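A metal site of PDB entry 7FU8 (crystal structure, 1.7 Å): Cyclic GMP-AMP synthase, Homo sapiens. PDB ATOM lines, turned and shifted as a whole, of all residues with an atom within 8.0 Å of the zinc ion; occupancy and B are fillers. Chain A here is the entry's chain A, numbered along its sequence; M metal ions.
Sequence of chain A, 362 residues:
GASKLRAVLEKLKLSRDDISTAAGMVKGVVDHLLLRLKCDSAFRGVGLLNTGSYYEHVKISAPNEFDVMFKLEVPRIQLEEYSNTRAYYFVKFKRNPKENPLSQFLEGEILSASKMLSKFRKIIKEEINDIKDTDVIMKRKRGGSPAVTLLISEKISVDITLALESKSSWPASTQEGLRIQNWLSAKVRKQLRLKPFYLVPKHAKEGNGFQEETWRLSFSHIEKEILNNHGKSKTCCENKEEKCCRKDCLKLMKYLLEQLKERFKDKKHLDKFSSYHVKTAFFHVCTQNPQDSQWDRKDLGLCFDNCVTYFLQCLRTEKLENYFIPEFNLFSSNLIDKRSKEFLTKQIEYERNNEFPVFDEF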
ATOM      1  N   LEU A 227       7.714  25.343  -1.845  1.00  0.00           N
ATOM      2  CA  LEU A 227       6.430  25.826  -1.340  1.00  0.00           C
ATOM      3  C   LEU A 227       5.456  24.676  -1.098  1.00  0.00           C
ATOM      4  O   LEU A 227       4.604  24.765  -0.206  1.00  0.00           O
ATOM      5  CB  LEU A 227       5.800  26.838  -2.302  1.00  0.00           C
ATOM      6  CG  LEU A 227       6.435  28.215  -2.267  1.00  0.00           C
ATOM      7  CD1 LEU A 227       5.991  28.999  -3.508  1.00  0.00           C
ATOM      8  CD2 LEU A 227       6.002  28.926  -0.994  1.00  0.00           C
ATOM      9  N   ASN A 229       6.460  21.755   0.030  1.00  0.00           N
ATOM     10  CA  ASN A 229       7.074  20.929   1.079  1.00  0.00           C
ATOM     11  C   ASN A 229       7.868  21.908   1.961  1.00  0.00           C
ATOM     12  O   ASN A 229       9.107  21.864   2.036  1.00  0.00           O
ATOM     13  CB  ASN A 229       7.948  19.817   0.490  1.00  0.00           C
ATOM     14  CG  ASN A 229       8.357  18.765   1.529  1.00  0.00           C
ATOM     15  OD1 ASN A 229       7.835  18.715   2.645  1.00  0.00           O
ATOM     16  ND2 ASN A 229       9.290  17.891   1.142  1.00  0.00           N
ATOM     17  N   HIS A 230       7.132  22.799   2.625  1.00  0.00           N
ATOM     18  CA  HIS A 230       7.673  24.064   3.152  1.00  0.00           C
ATOM     19  C   HIS A 230       7.896  24.071   4.656  1.00  0.00           C
ATOM     20  O   HIS A 230       8.425  25.074   5.172  1.00  0.00           O
ATOM     21  CB  HIS A 230       6.717  25.229   2.813  1.00  0.00           C
ATOM     22  CG  HIS A 230       5.363  25.053   3.407  1.00  0.00           C
ATOM     23  ND1 HIS A 230       4.238  24.819   2.647  1.00  0.00           N
ATOM     24  CD2 HIS A 230       4.961  24.969   4.708  1.00  0.00           C
ATOM     25  CE1 HIS A 230       3.197  24.642   3.437  1.00  0.00           C
ATOM     26  NE2 HIS A 230       3.611  24.712   4.702  1.00  0.00           N
ATOM     27  N   GLY A 231       7.433  23.054   5.394  1.00  0.00           N
ATOM     28  CA  GLY A 231       7.532  23.124   6.838  1.00  0.00           C
ATOM     29  C   GLY A 231       8.841  22.596   7.367  1.00  0.00           C
ATOM     30  O   GLY A 231       9.519  21.803   6.716  1.00  0.00           O
ATOM     31  N   LYS A 232       9.204  23.024   8.598  1.00  0.00           N
ATOM     32  CA  LYS A 232      10.177  22.248   9.342  1.00  0.00           C
ATOM     33  C   LYS A 232       9.603  20.865   9.633  1.00  0.00           C
ATOM     34  O   LYS A 232      10.277  19.842   9.448  1.00  0.00           O
ATOM     35  CB  LYS A 232      10.574  22.944  10.659  1.00  0.00           C
ATOM     36  CG  LYS A 232      11.564  22.096  11.456  1.00  0.00           C
ATOM     37  CD  LYS A 232      12.292  22.861  12.554  1.00  0.00           C
ATOM     38  CE  LYS A 232      13.148  23.999  11.976  1.00  0.00           C
ATOM     39  NZ  LYS A 232      14.292  23.474  11.178  1.00  0.00           N
ATOM     40  N   SER A 233       8.329  20.818  10.026  1.00  0.00           N
ATOM     41  CA  SER A 233       7.633  19.540  10.166  1.00  0.00           C
ATOM     42  C   SER A 233       7.364  18.908   8.811  1.00  0.00           C
ATOM     43  O   SER A 233       6.911  19.579   7.870  1.00  0.00           O
ATOM     44  CB  SER A 233       6.284  19.739  10.876  1.00  0.00           C
ATOM     45  OG  SER A 233       5.556  18.510  10.876  1.00  0.00           O
ATOM     46  N   THR A 235       4.929  16.998   8.322  1.00  0.00           N
ATOM     47  CA  THR A 235       3.488  17.022   8.146  1.00  0.00           C
ATOM     48  C   THR A 235       2.897  18.435   8.242  1.00  0.00           C
ATOM     49  O   THR A 235       1.700  18.587   8.488  1.00  0.00           O
ATOM     50  CB  THR A 235       2.832  16.103   9.179  1.00  0.00           C
ATOM     51  OG1 THR A 235       3.225  16.493  10.510  1.00  0.00           O
ATOM     52  CG2 THR A 235       3.268  14.651   8.924  1.00  0.00           C
ATOM     53  N   CYS A 236       3.716  19.461   8.024  1.00  0.00           N
ATOM     54  CA  CYS A 236       3.185  20.831   8.033  1.00  0.00           C
ATOM     55  C   CYS A 236       2.095  20.968   6.968  1.00  0.00           C
ATOM     56  O   CYS A 236       2.294  20.598   5.808  1.00  0.00           O
ATOM     57  CB  CYS A 236       4.308  21.851   7.789  1.00  0.00           C
ATOM     58  SG  CYS A 236       3.809  23.598   8.096  1.00  0.00           S
ATOM     59  N   CYS A 237       0.940  21.498   7.387  1.00  0.00           N
ATOM     60  CA  CYS A 237      -0.244  21.699   6.539  1.00  0.00           C
ATOM     61  C   CYS A 237      -0.815  20.377   6.019  1.00  0.00           C
ATOM     62  O   CYS A 237      -1.392  20.315   4.929  1.00  0.00           O
ATOM     63  CB  CYS A 237       0.050  22.640   5.376  1.00  0.00           C
ATOM     64  SG  CYS A 237       0.330  24.350   5.921  1.00  0.00           S
ATOM     65  N   GLU A 238      -0.664  19.294   6.779  1.00  0.00           N
ATOM     66  CA  GLU A 238      -1.284  18.022   6.428  1.00  0.00           C
ATOM     67  C   GLU A 238      -2.237  17.499   7.504  1.00  0.00           C
ATOM     68  O   GLU A 238      -2.767  16.397   7.364  1.00  0.00           O
ATOM     69  CB  GLU A 238      -0.186  16.996   6.091  1.00  0.00           C
ATOM     70  CG  GLU A 238       0.637  17.465   4.895  1.00  0.00           C
ATOM     71  CD  GLU A 238       1.761  16.536   4.517  1.00  0.00           C
ATOM     72  OE1 GLU A 238       1.739  15.365   4.951  1.00  0.00           O
ATOM     73  OE2 GLU A 238       2.681  16.992   3.768  1.00  0.00           O
ATOM     74  N   GLU A 242      -1.590  21.520  12.435  1.00  0.00           N
ATOM     75  CA  GLU A 242      -0.344  21.915  11.800  1.00  0.00           C
ATOM     76  C   GLU A 242      -0.619  22.761  10.570  1.00  0.00           C
ATOM     77  O   GLU A 242       0.036  22.602   9.534  1.00  0.00           O
ATOM     78  CB  GLU A 242       0.495  20.698  11.404  1.00  0.00           C
ATOM     79  CG  GLU A 242       1.063  19.924  12.564  1.00  0.00           C
ATOM     80  CD  GLU A 242       2.170  18.997  12.121  1.00  0.00           C
ATOM     81  OE1 GLU A 242       3.287  19.508  11.828  1.00  0.00           O
ATOM     82  OE2 GLU A 242       1.910  17.776  12.036  1.00  0.00           O
ATOM     83  N   LYS A 243      -1.600  23.654  10.664  1.00  0.00           N
ATOM     84  CA  LYS A 243      -1.898  24.591   9.591  1.00  0.00           C
ATOM     85  C   LYS A 243      -1.110  25.885   9.811  1.00  0.00           C
ATOM     86  O   LYS A 243      -1.313  26.584  10.803  1.00  0.00           O
ATOM     87  CB  LYS A 243      -3.403  24.830   9.518  1.00  0.00           C
ATOM     88  CG  LYS A 243      -4.048  24.053   8.407  1.00  0.00           C
ATOM     89  CD  LYS A 243      -3.486  24.541   7.070  1.00  0.00           C
ATOM     90  CE  LYS A 243      -3.923  23.630   5.931  1.00  0.00           C
ATOM     91  NZ  LYS A 243      -4.006  24.340   4.623  1.00  0.00           N
ATOM     92  N   CYS A 244      -0.163  26.168   8.913  1.00  0.00           N
ATOM     93  CA  CYS A 244       0.679  27.347   8.998  1.00  0.00           C
ATOM     94  C   CYS A 244       0.214  28.396   7.990  1.00  0.00           C
ATOM     95  O   CYS A 244      -0.601  28.115   7.097  1.00  0.00           O
ATOM     96  CB  CYS A 244       2.162  27.001   8.780  1.00  0.00           C
ATOM     97  SG  CYS A 244       2.766  26.897   7.056  1.00  0.00           S
ATOM     98  N   CYS A 245       0.737  29.611   8.116  1.00  0.00           N
ATOM     99  CA  CYS A 245       0.326  30.688   7.216  1.00  0.00           C
ATOM    100  C   CYS A 245       1.456  31.155   6.296  1.00  0.00           C
ATOM    101  O   CYS A 245       1.438  32.314   5.868  1.00  0.00           O
ATOM    102  CB  CYS A 245      -0.217  31.882   7.999  1.00  0.00           C
ATOM    103  SG  CYS A 245       1.001  32.662   9.109  1.00  0.00           S
ATOM    104  N   ARG A 246       2.418  30.280   5.967  1.00  0.00           N
ATOM    105  CA  ARG A 246       3.484  30.673   5.029  1.00  0.00           C
ATOM    106  C   ARG A 246       2.908  31.048   3.660  1.00  0.00           C
ATOM    107  O   ARG A 246       3.178  32.153   3.142  1.00  0.00           O
ATOM    108  CB  ARG A 246       4.519  29.530   4.881  1.00  0.00           C
ATOM    109  CG  ARG A 246       5.492  29.409   6.064  1.00  0.00           C
ATOM    110  CD  ARG A 246       6.511  28.302   5.788  1.00  0.00           C
ATOM    111  NE  ARG A 246       7.458  28.063   6.881  1.00  0.00           N
ATOM    112  CZ  ARG A 246       7.268  27.195   7.878  1.00  0.00           C
ATOM    113  NH1 ARG A 246       6.134  26.515   7.994  1.00  0.00           N
ATOM    114  NH2 ARG A 246       8.236  27.023   8.769  1.00  0.00           N
ATOM    115  N   LYS A 247       2.125  30.159   3.050  1.00  0.00           N
ATOM    116  CA  LYS A 247       1.593  30.430   1.726  1.00  0.00           C
ATOM    117  C   LYS A 247       0.698  31.659   1.723  1.00  0.00           C
ATOM    118  O   LYS A 247       0.718  32.455   0.779  1.00  0.00           O
ATOM    119  CB  LYS A 247       0.829  29.217   1.204  1.00  0.00           C
ATOM    120  CG  LYS A 247       1.755  28.102   0.658  1.00  0.00           C
ATOM    121  CD  LYS A 247       0.909  26.953   0.112  1.00  0.00           C
ATOM    122  CE  LYS A 247       1.757  26.021  -0.727  1.00  0.00           C
ATOM    123  NZ  LYS A 247       1.053  24.750  -1.025  1.00  0.00           N
ATOM    124  N   ASP A 292       7.930  26.170  12.497  1.00  0.00           N
ATOM    125  CA  ASP A 292       6.522  26.261  12.110  1.00  0.00           C
ATOM    126  C   ASP A 292       5.709  27.084  13.110  1.00  0.00           C
ATOM    127  O   ASP A 292       4.757  27.770  12.722  1.00  0.00           O
ATOM    128  CB  ASP A 292       5.923  24.856  11.950  1.00  0.00           C
ATOM    129  CG  ASP A 292       6.621  24.037  10.852  1.00  0.00           C
ATOM    130  OD1 ASP A 292       7.329  24.593   9.984  1.00  0.00           O
ATOM    131  OD2 ASP A 292       6.436  22.803  10.857  1.00  0.00           O
ATOM    132  N   TRP A 295       4.816  30.549  12.373  1.00  0.00           N
ATOM    133  CA  TRP A 295       3.928  30.738  11.243  1.00  0.00           C
ATOM    134  C   TRP A 295       2.553  30.198  11.594  1.00  0.00           C
ATOM    135  O   TRP A 295       1.836  29.698  10.728  1.00  0.00           O
ATOM    136  CB  TRP A 295       4.468  30.056   9.989  1.00  0.00           C
ATOM    137  CG  TRP A 295       5.767  30.616   9.521  1.00  0.00           C
ATOM    138  CD1 TRP A 295       7.026  30.146   9.818  1.00  0.00           C
ATOM    139  CD2 TRP A 295       5.967  31.788   8.701  1.00  0.00           C
ATOM    140  NE1 TRP A 295       7.985  30.945   9.212  1.00  0.00           N
ATOM    141  CE2 TRP A 295       7.363  31.957   8.521  1.00  0.00           C
ATOM    142  CE3 TRP A 295       5.085  32.704   8.080  1.00  0.00           C
ATOM    143  CZ2 TRP A 295       7.910  32.990   7.755  1.00  0.00           C
ATOM    144  CZ3 TRP A 295       5.637  33.749   7.310  1.00  0.00           C
ATOM    145  CH2 TRP A 295       7.031  33.873   7.140  1.00  0.00           C
HETATM  146 ZN    ZN M   1       2.564  24.650   6.424  1.00  0.00          ZN
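Four residues have an atom within 4 Å of the zinc ion: His 230, Cys 236, Cys 237 and Cys 244.
The side-chain sulfur (SG) of Cys 244 lies close to the guanidinium group (NH1) of Arg 246 (3.5 Å).
The side-chain sulfur (SG) of Cys 236 sits close to the guanidinium group (NH1) of Arg 246 (3.7 Å).
A ring nitrogen (ND1) of His 230 is in hydrogen-bond range of the backbone carbonyl oxygen (O) of Leu 227 (2.9 Å).
O of Glu 242 sits at hydrogen-bond distance from N of Cys 237 (2.6 Å).
NE2 of His 230 is bound to the zinc ion.
The side-chain sulfur (SG) of Cys 237 is bound to the zinc ion (2.3 Å).
SG of Cys 236 is bound to the zinc ion (2.3 Å).
SG of Cys 244 binds the zinc ion (2.3 Å).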
